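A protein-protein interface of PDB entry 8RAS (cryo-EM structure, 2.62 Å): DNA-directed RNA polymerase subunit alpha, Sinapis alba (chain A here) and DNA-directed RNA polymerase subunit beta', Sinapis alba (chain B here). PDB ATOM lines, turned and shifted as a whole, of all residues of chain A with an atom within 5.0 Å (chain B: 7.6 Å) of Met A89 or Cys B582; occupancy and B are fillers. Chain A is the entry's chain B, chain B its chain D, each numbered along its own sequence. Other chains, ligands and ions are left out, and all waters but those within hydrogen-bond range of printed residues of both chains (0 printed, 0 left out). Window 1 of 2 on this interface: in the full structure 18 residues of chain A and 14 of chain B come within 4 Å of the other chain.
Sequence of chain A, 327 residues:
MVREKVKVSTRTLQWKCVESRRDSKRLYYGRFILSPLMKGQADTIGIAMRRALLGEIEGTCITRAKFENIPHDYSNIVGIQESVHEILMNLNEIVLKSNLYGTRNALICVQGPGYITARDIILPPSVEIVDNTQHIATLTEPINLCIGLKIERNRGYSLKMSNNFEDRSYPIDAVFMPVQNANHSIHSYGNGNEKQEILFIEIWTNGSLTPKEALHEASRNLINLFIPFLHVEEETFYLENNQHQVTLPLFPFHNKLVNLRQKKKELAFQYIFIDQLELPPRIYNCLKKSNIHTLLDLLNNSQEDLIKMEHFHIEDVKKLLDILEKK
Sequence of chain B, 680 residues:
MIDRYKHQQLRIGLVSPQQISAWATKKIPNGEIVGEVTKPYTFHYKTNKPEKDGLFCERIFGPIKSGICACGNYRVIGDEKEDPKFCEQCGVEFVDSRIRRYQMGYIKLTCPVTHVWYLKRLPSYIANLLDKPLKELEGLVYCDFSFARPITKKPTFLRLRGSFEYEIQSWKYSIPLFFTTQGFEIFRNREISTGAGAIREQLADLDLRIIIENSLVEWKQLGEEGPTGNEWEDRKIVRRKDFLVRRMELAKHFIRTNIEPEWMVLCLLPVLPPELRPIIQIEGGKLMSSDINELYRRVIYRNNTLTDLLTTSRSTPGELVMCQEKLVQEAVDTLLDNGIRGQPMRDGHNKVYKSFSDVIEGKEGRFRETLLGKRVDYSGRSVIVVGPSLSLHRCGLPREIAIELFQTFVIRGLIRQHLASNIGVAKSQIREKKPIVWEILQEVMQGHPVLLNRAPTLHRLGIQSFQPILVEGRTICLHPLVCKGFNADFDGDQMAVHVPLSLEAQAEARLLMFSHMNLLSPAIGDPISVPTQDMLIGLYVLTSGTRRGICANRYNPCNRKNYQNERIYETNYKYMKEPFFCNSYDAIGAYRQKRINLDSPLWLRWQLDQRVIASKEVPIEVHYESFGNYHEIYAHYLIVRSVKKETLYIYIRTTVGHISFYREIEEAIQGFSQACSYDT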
ATOM      1  N   HIS A  85       0.729 -15.970  20.079  1.00  0.00           N
ATOM      2  CA  HIS A  85       0.117 -15.555  18.821  1.00  0.00           C
ATOM      3  C   HIS A  85       0.990 -15.941  17.634  1.00  0.00           C
ATOM      4  O   HIS A  85       0.483 -16.373  16.592  1.00  0.00           O
ATOM      5  CB  HIS A  85      -0.137 -14.049  18.840  1.00  0.00           C
ATOM      6  CG  HIS A  85      -0.913 -13.550  17.662  1.00  0.00           C
ATOM      7  ND1 HIS A  85      -2.273 -13.734  17.536  1.00  0.00           N
ATOM      8  CD2 HIS A  85      -0.522 -12.869  16.559  1.00  0.00           C
ATOM      9  CE1 HIS A  85      -2.686 -13.190  16.405  1.00  0.00           C
ATOM     10  NE2 HIS A  85      -1.643 -12.658  15.793  1.00  0.00           N
ATOM     11  N   GLU A  86       2.309 -15.792  17.774  1.00  0.00           N
ATOM     12  CA  GLU A  86       3.219 -16.217  16.717  1.00  0.00           C
ATOM     13  C   GLU A  86       3.144 -17.722  16.498  1.00  0.00           C
ATOM     14  O   GLU A  86       3.195 -18.195  15.357  1.00  0.00           O
ATOM     15  CB  GLU A  86       4.647 -15.791  17.055  1.00  0.00           C
ATOM     16  CG  GLU A  86       5.109 -14.551  16.317  1.00  0.00           C
ATOM     17  CD  GLU A  86       5.757 -14.876  14.987  1.00  0.00           C
ATOM     18  OE1 GLU A  86       6.188 -16.033  14.804  1.00  0.00           O
ATOM     19  OE2 GLU A  86       5.830 -13.977  14.124  1.00  0.00           O
ATOM     20  N   ILE A  87       3.023 -18.491  17.582  1.00  0.00           N
ATOM     21  CA  ILE A  87       2.895 -19.941  17.458  1.00  0.00           C
ATOM     22  C   ILE A  87       1.611 -20.303  16.722  1.00  0.00           C
ATOM     23  O   ILE A  87       1.603 -21.185  15.856  1.00  0.00           O
ATOM     24  CB  ILE A  87       2.965 -20.605  18.844  1.00  0.00           C
ATOM     25  CG1 ILE A  87       4.412 -20.656  19.336  1.00  0.00           C
ATOM     26  CG2 ILE A  87       2.379 -22.006  18.799  1.00  0.00           C
ATOM     27  CD1 ILE A  87       4.562 -21.197  20.737  1.00  0.00           C
ATOM     28  N   LEU A  88       0.506 -19.633  17.056  1.00  0.00           N
ATOM     29  CA  LEU A  88      -0.753 -19.899  16.364  1.00  0.00           C
ATOM     30  C   LEU A  88      -0.659 -19.542  14.886  1.00  0.00           C
ATOM     31  O   LEU A  88      -1.160 -20.279  14.027  1.00  0.00           O
ATOM     32  CB  LEU A  88      -1.892 -19.131  17.032  1.00  0.00           C
ATOM     33  CG  LEU A  88      -2.155 -19.455  18.501  1.00  0.00           C
ATOM     34  CD1 LEU A  88      -3.019 -18.381  19.142  1.00  0.00           C
ATOM     35  CD2 LEU A  88      -2.803 -20.820  18.639  1.00  0.00           C
ATOM     36  N   MET A  89      -0.017 -18.414  14.570  1.00  0.00           N
ATOM     37  CA  MET A  89       0.159 -18.031  13.173  1.00  0.00           C
ATOM     38  C   MET A  89       1.004 -19.056  12.427  1.00  0.00           C
ATOM     39  O   MET A  89       0.727 -19.373  11.265  1.00  0.00           O
ATOM     40  CB  MET A  89       0.795 -16.643  13.086  1.00  0.00           C
ATOM     41  CG  MET A  89      -0.187 -15.491  13.250  1.00  0.00           C
ATOM     42  SD  MET A  89      -0.783 -14.825  11.683  1.00  0.00           S
ATOM     43  CE  MET A  89      -2.276 -15.784  11.452  1.00  0.00           C
ATOM     44  N   ASN A  90       2.047 -19.577  13.077  1.00  0.00           N
ATOM     45  CA  ASN A  90       2.853 -20.630  12.468  1.00  0.00           C
ATOM     46  C   ASN A  90       2.031 -21.892  12.240  1.00  0.00           C
ATOM     47  O   ASN A  90       2.162 -22.551  11.203  1.00  0.00           O
ATOM     48  CB  ASN A  90       4.065 -20.936  13.346  1.00  0.00           C
ATOM     49  CG  ASN A  90       5.172 -19.915  13.190  1.00  0.00           C
ATOM     50  OD1 ASN A  90       5.406 -19.398  12.099  1.00  0.00           O
ATOM     51  ND2 ASN A  90       5.860 -19.620  14.284  1.00  0.00           N
ATOM     52  N   LEU A  91       1.185 -22.248  13.209  1.00  0.00           N
ATOM     53  CA  LEU A  91       0.346 -23.434  13.076  1.00  0.00           C
ATOM     54  C   LEU A  91      -0.660 -23.289  11.943  1.00  0.00           C
ATOM     55  O   LEU A  91      -0.988 -24.276  11.277  1.00  0.00           O
ATOM     56  CB  LEU A  91      -0.381 -23.717  14.390  1.00  0.00           C
ATOM     57  CG  LEU A  91       0.469 -24.226  15.554  1.00  0.00           C
ATOM     58  CD1 LEU A  91      -0.349 -24.256  16.834  1.00  0.00           C
ATOM     59  CD2 LEU A  91       1.034 -25.599  15.243  1.00  0.00           C
ATOM     60  N   ASN A  92      -1.164 -22.074  11.715  1.00  0.00           N
ATOM     61  CA  ASN A  92      -2.120 -21.857  10.637  1.00  0.00           C
ATOM     62  C   ASN A  92      -1.513 -22.100   9.261  1.00  0.00           C
ATOM     63  O   ASN A  92      -2.257 -22.300   8.295  1.00  0.00           O
ATOM     64  CB  ASN A  92      -2.679 -20.436  10.710  1.00  0.00           C
ATOM     65  CG  ASN A  92      -3.988 -20.288   9.966  1.00  0.00           C
ATOM     66  OD1 ASN A  92      -4.595 -21.275   9.552  1.00  0.00           O
ATOM     67  ND2 ASN A  92      -4.431 -19.050   9.792  1.00  0.00           N
ATOM     68  N   GLU A  93      -0.188 -22.094   9.146  1.00  0.00           N
ATOM     69  CA  GLU A  93       0.487 -22.231   7.863  1.00  0.00           C
ATOM     70  C   GLU A  93       0.793 -23.676   7.490  1.00  0.00           C
ATOM     71  O   GLU A  93       1.287 -23.920   6.385  1.00  0.00           O
ATOM     72  CB  GLU A  93       1.790 -21.425   7.866  1.00  0.00           C
ATOM     73  CG  GLU A  93       1.607 -19.940   7.627  1.00  0.00           C
ATOM     74  CD  GLU A  93       2.626 -19.376   6.658  1.00  0.00           C
ATOM     75  OE1 GLU A  93       3.242 -20.169   5.914  1.00  0.00           O
ATOM     76  OE2 GLU A  93       2.814 -18.142   6.638  1.00  0.00           O
ATOM     77  N   PRO B 579      -9.747 -10.237  11.351  1.00  0.00           N
ATOM     78  CA  PRO B 579      -8.945 -11.432  11.072  1.00  0.00           C
ATOM     79  C   PRO B 579      -7.469 -11.114  10.893  1.00  0.00           C
ATOM     80  O   PRO B 579      -7.086 -10.035  10.435  1.00  0.00           O
ATOM     81  CB  PRO B 579      -9.555 -11.969   9.772  1.00  0.00           C
ATOM     82  CG  PRO B 579     -10.190 -10.784   9.136  1.00  0.00           C
ATOM     83  CD  PRO B 579     -10.687  -9.930  10.261  1.00  0.00           C
ATOM     84  N   PHE B 580      -6.638 -12.083  11.266  1.00  0.00           N
ATOM     85  CA  PHE B 580      -5.200 -12.039  11.044  1.00  0.00           C
ATOM     86  C   PHE B 580      -4.847 -13.022   9.938  1.00  0.00           C
ATOM     87  O   PHE B 580      -5.269 -14.182   9.979  1.00  0.00           O
ATOM     88  CB  PHE B 580      -4.432 -12.388  12.319  1.00  0.00           C
ATOM     89  CG  PHE B 580      -4.090 -11.201  13.170  1.00  0.00           C
ATOM     90  CD1 PHE B 580      -5.045 -10.618  13.985  1.00  0.00           C
ATOM     91  CD2 PHE B 580      -2.810 -10.677  13.166  1.00  0.00           C
ATOM     92  CE1 PHE B 580      -4.731  -9.529  14.771  1.00  0.00           C
ATOM     93  CE2 PHE B 580      -2.490  -9.589  13.953  1.00  0.00           C
ATOM     94  CZ  PHE B 580      -3.451  -9.014  14.755  1.00  0.00           C
ATOM     95  N   PHE B 581      -4.077 -12.562   8.958  1.00  0.00           N
ATOM     96  CA  PHE B 581      -3.698 -13.379   7.816  1.00  0.00           C
ATOM     97  C   PHE B 581      -2.184 -13.502   7.746  1.00  0.00           C
ATOM     98  O   PHE B 581      -1.461 -12.515   7.919  1.00  0.00           O
ATOM     99  CB  PHE B 581      -4.240 -12.789   6.513  1.00  0.00           C
ATOM    100  CG  PHE B 581      -5.730 -12.901   6.376  1.00  0.00           C
ATOM    101  CD1 PHE B 581      -6.318 -14.103   6.023  1.00  0.00           C
ATOM    102  CD2 PHE B 581      -6.544 -11.806   6.603  1.00  0.00           C
ATOM    103  CE1 PHE B 581      -7.687 -14.209   5.897  1.00  0.00           C
ATOM    104  CE2 PHE B 581      -7.913 -11.907   6.478  1.00  0.00           C
ATOM    105  CZ  PHE B 581      -8.485 -13.108   6.125  1.00  0.00           C
ATOM    106  N   CYS B 582      -1.710 -14.725   7.497  1.00  0.00           N
ATOM    107  CA  CYS B 582      -0.273 -14.962   7.408  1.00  0.00           C
ATOM    108  C   CYS B 582       0.334 -14.252   6.205  1.00  0.00           C
ATOM    109  O   CYS B 582       1.430 -13.687   6.299  1.00  0.00           O
ATOM    110  CB  CYS B 582       0.006 -16.461   7.340  1.00  0.00           C
ATOM    111  SG  CYS B 582      -0.801 -17.429   8.632  1.00  0.00           S
ATOM    112  N   ASN B 583      -0.358 -14.267   5.070  1.00  0.00           N
ATOM    113  CA  ASN B 583       0.149 -13.645   3.857  1.00  0.00           C
ATOM    114  C   ASN B 583      -1.022 -13.109   3.046  1.00  0.00           C
ATOM    115  O   ASN B 583      -2.186 -13.403   3.325  1.00  0.00           O
ATOM    116  CB  ASN B 583       0.991 -14.628   3.036  1.00  0.00           C
ATOM    117  CG  ASN B 583       0.365 -16.005   2.955  1.00  0.00           C
ATOM    118  OD1 ASN B 583       0.326 -16.741   3.940  1.00  0.00           O
ATOM    119  ND2 ASN B 583      -0.132 -16.360   1.780  1.00  0.00           N
ATOM    120  N   SER B 584      -0.692 -12.305   2.031  1.00  0.00           N
ATOM    121  CA  SER B 584      -1.721 -11.670   1.213  1.00  0.00           C
ATOM    122  C   SER B 584      -2.542 -12.692   0.438  1.00  0.00           C
ATOM    123  O   SER B 584      -3.732 -12.466   0.179  1.00  0.00           O
ATOM    124  CB  SER B 584      -1.077 -10.678   0.248  1.00  0.00           C
ATOM    125  OG  SER B 584      -0.393 -11.358  -0.789  1.00  0.00           O
ATOM    126  N   TYR B 585      -1.926 -13.811   0.051  1.00  0.00           N
ATOM    127  CA  TYR B 585      -2.659 -14.844  -0.672  1.00  0.00           C
ATOM    128  C   TYR B 585      -3.788 -15.406   0.179  1.00  0.00           C
ATOM    129  O   TYR B 585      -4.884 -15.664  -0.328  1.00  0.00           O
ATOM    130  CB  TYR B 585      -1.708 -15.958  -1.111  1.00  0.00           C
ATOM    131  CG  TYR B 585      -0.454 -15.460  -1.789  1.00  0.00           C
ATOM    132  CD1 TYR B 585      -0.511 -14.849  -3.033  1.00  0.00           C
ATOM    133  CD2 TYR B 585       0.786 -15.598  -1.184  1.00  0.00           C
ATOM    134  CE1 TYR B 585       0.631 -14.389  -3.655  1.00  0.00           C
ATOM    135  CE2 TYR B 585       1.933 -15.143  -1.797  1.00  0.00           C
ATOM    136  CZ  TYR B 585       1.851 -14.540  -3.033  1.00  0.00           C
ATOM    137  OH  TYR B 585       2.995 -14.084  -3.647  1.00  0.00           O
ATOM    138  N   ASP B 586      -3.542 -15.592   1.477  1.00  0.00           N
ATOM    139  CA  ASP B 586      -4.596 -16.060   2.372  1.00  0.00           C
ATOM    140  C   ASP B 586      -5.750 -15.067   2.434  1.00  0.00           C
ATOM    141  O   ASP B 586      -6.921 -15.463   2.421  1.00  0.00           O
ATOM    142  CB  ASP B 586      -4.024 -16.304   3.768  1.00  0.00           C
ATOM    143  CG  ASP B 586      -3.408 -17.680   3.914  1.00  0.00           C
ATOM    144  OD1 ASP B 586      -3.809 -18.596   3.166  1.00  0.00           O
ATOM    145  OD2 ASP B 586      -2.520 -17.845   4.777  1.00  0.00           O
ATOM    146  N   ALA B 587      -5.438 -13.771   2.502  1.00  0.00           N
ATOM    147  CA  ALA B 587      -6.484 -12.756   2.564  1.00  0.00           C
ATOM    148  C   ALA B 587      -7.316 -12.731   1.289  1.00  0.00           C
ATOM    149  O   ALA B 587      -8.550 -12.663   1.342  1.00  0.00           O
ATOM    150  CB  ALA B 587      -5.867 -11.383   2.824  1.00  0.00           C
ATOM    151  N   TRP B 603      -5.684  -7.650   9.514  1.00  0.00           N
ATOM    152  CA  TRP B 603      -4.280  -7.511   9.866  1.00  0.00           C
ATOM    153  C   TRP B 603      -3.453  -8.444   8.995  1.00  0.00           C
ATOM    154  O   TRP B 603      -3.738  -9.643   8.919  1.00  0.00           O
ATOM    155  CB  TRP B 603      -4.052  -7.817  11.346  1.00  0.00           C
ATOM    156  CG  TRP B 603      -4.605  -6.775  12.261  1.00  0.00           C
ATOM    157  CD1 TRP B 603      -5.826  -6.782  12.865  1.00  0.00           C
ATOM    158  CD2 TRP B 603      -3.957  -5.569  12.679  1.00  0.00           C
ATOM    159  NE1 TRP B 603      -5.980  -5.655  13.634  1.00  0.00           N
ATOM    160  CE2 TRP B 603      -4.846  -4.894  13.536  1.00  0.00           C
ATOM    161  CE3 TRP B 603      -2.711  -4.994  12.411  1.00  0.00           C
ATOM    162  CZ2 TRP B 603      -4.529  -3.675  14.128  1.00  0.00           C
ATOM    163  CZ3 TRP B 603      -2.400  -3.785  12.999  1.00  0.00           C
ATOM    164  CH2 TRP B 603      -3.304  -3.139  13.847  1.00  0.00           C
ATOM    165  N   LEU B 604      -2.437  -7.892   8.342  1.00  0.00           N
ATOM    166  CA  LEU B 604      -1.584  -8.639   7.430  1.00  0.00           C
ATOM    167  C   LEU B 604      -0.189  -8.761   8.021  1.00  0.00           C
ATOM    168  O   LEU B 604       0.436  -7.753   8.359  1.00  0.00           O
ATOM    169  CB  LEU B 604      -1.513  -7.953   6.065  1.00  0.00           C
ATOM    170  CG  LEU B 604      -0.686  -8.685   5.010  1.00  0.00           C
ATOM    171  CD1 LEU B 604      -1.260 -10.066   4.757  1.00  0.00           C
ATOM    172  CD2 LEU B 604      -0.612  -7.883   3.725  1.00  0.00           C
ATOM    173  N   ARG B 605       0.297  -9.994   8.134  1.00  0.00           N
ATOM    174  CA  ARG B 605       1.665 -10.212   8.583  1.00  0.00           C
ATOM    175  C   ARG B 605       2.639  -9.694   7.534  1.00  0.00           C
ATOM    176  O   ARG B 605       2.572 -10.081   6.364  1.00  0.00           O
ATOM    177  CB  ARG B 605       1.909 -11.695   8.849  1.00  0.00           C
ATOM    178  CG  ARG B 605       3.314 -12.009   9.328  1.00  0.00           C
ATOM    179  CD  ARG B 605       3.327 -13.220  10.240  1.00  0.00           C
ATOM    180  NE  ARG B 605       3.377 -14.467   9.484  1.00  0.00           N
ATOM    181  CZ  ARG B 605       3.755 -15.632   9.989  1.00  0.00           C
ATOM    182  NH1 ARG B 605       4.128 -15.751  11.252  1.00  0.00           N
ATOM    183  NH2 ARG B 605       3.762 -16.706   9.205  1.00  0.00           N
ATOM    184  N   TRP B 606       3.543  -8.817   7.956  1.00  0.00           N
ATOM    185  CA  TRP B 606       4.519  -8.203   7.069  1.00  0.00           C
ATOM    186  C   TRP B 606       5.889  -8.803   7.341  1.00  0.00           C
ATOM    187  O   TRP B 606       6.363  -8.787   8.481  1.00  0.00           O
ATOM    188  CB  TRP B 606       4.551  -6.686   7.262  1.00  0.00           C
ATOM    189  CG  TRP B 606       5.098  -5.934   6.090  1.00  0.00           C
ATOM    190  CD1 TRP B 606       6.176  -5.102   6.084  1.00  0.00           C
ATOM    191  CD2 TRP B 606       4.582  -5.933   4.753  1.00  0.00           C
ATOM    192  NE1 TRP B 606       6.371  -4.587   4.827  1.00  0.00           N
ATOM    193  CE2 TRP B 606       5.405  -5.082   3.991  1.00  0.00           C
ATOM    194  CE3 TRP B 606       3.507  -6.571   4.127  1.00  0.00           C
ATOM    195  CZ2 TRP B 606       5.188  -4.852   2.636  1.00  0.00           C
ATOM    196  CZ3 TRP B 606       3.295  -6.341   2.782  1.00  0.00           C
ATOM    197  CH2 TRP B 606       4.130  -5.490   2.050  1.00  0.00           C
ATOM    198  N   GLN B 607       6.522  -9.332   6.293  1.00  0.00           N
ATOM    199  CA  GLN B 607       7.840  -9.945   6.405  1.00  0.00           C
ATOM    200  C   GLN B 607       8.882  -9.209   5.573  1.00  0.00           C
ATOM    201  O   GLN B 607       9.908  -9.792   5.208  1.00  0.00           O
ATOM    202  CB  GLN B 607       7.778 -11.421   6.006  1.00  0.00           C
ATOM    203  CG  GLN B 607       7.435 -12.348   7.158  1.00  0.00           C
ATOM    204  CD  GLN B 607       6.711 -13.598   6.703  1.00  0.00           C
ATOM    205  OE1 GLN B 607       5.486 -13.610   6.586  1.00  0.00           O
ATOM    206  NE2 GLN B 607       7.466 -14.658   6.443  1.00  0.00           N
ATOM    207  N   TYR B 651       2.750  -6.062  11.599  1.00  0.00           N
ATOM    208  CA  TYR B 651       1.424  -6.390  11.095  1.00  0.00           C
ATOM    209  C   TYR B 651       0.780  -5.119  10.568  1.00  0.00           C
ATOM    210  O   TYR B 651       0.701  -4.121  11.287  1.00  0.00           O
ATOM    211  CB  TYR B 651       0.551  -7.020  12.185  1.00  0.00           C
ATOM    212  CG  TYR B 651       1.146  -8.267  12.793  1.00  0.00           C
ATOM    213  CD1 TYR B 651       1.997  -8.191  13.886  1.00  0.00           C
ATOM    214  CD2 TYR B 651       0.860  -9.521  12.272  1.00  0.00           C
ATOM    215  CE1 TYR B 651       2.546  -9.327  14.444  1.00  0.00           C
ATOM    216  CE2 TYR B 651       1.403 -10.662  12.823  1.00  0.00           C
ATOM    217  CZ  TYR B 651       2.246 -10.559  13.909  1.00  0.00           C
ATOM    218  OH  TYR B 651       2.791 -11.694  14.464  1.00  0.00           O
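The guanidinium group (NH1) of Arg B605 lies within salt-bridge range of the side-chain carboxylate (OE2) of Glu A86, at 3.8 Å. The backbone carbonyl oxygen (O) of Met A89 lies close to the side-chain sulfur (SG) of Cys B582 (3.6 Å). OE2 of Glu A93 lies within salt-bridge range of NH2 of Arg B605, 3.1 Å away.
ND2 of Asn A90 is in hydrogen-bond range of O of Glu A86. O of Phe B581 is in hydrogen-bond range of N of Arg B605, 3.1 Å away. The side-chain amide oxygen (OD1) of Asn B583 sits close to the side-chain carboxylate (OD2) of Asp B586 (3.2 Å).
Among the printed residues, merely in contact across the chains: Glu A93 with Cys B582 (3.3 Å), His A85 with Phe B580 (3.5 Å), Met A89 with Phe B580 (3.7 Å), Glu A86 with Tyr B651 (3.8 Å), Met A89 with Arg B605 (3.9 Å), Glu A93 with Asn B583 (3.9 Å) and Asn A90 with Arg B605 (3.96 Å).
Met A89 touches three residues of chain B. Printed residues of chain A within 4 Å of Cys B582: Met A89 and Glu A93. Printed residues of chain B within 4 Å of Glu A86: Arg B605 (3.8 Å) and Tyr B651 (3.8 Å). Printed residues of chain A within 4 Å of Phe B580: His A85 and Met A89. Pro B579 touches none of the printed residues of chain A. Phe B581 touches none of the printed residues of chain A.
Of the 9 printed residues of chain A, 5 touch a printed residue of chain B. Printed residues of chain A that touch a printed residue of chain B: His A85, Glu A86, Met A89, Asn A90 and Glu A93. Of the 15 printed residues of chain B, 5 touch a printed residue of chain A. Hydrophobic or aromatic side chains of chain B that line the printed part of chain A: Phe B580 and Tyr B651. Among the printed residues, 10 pairs touch across the chains. Among the printed residues, Asp or Glu carboxylates within 4 Å of a Lys or Arg side-chain nitrogen of the other chain: Glu A86 with Arg B605 (3.8 Å) and Glu A93 with Arg B605 (3.1 Å).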
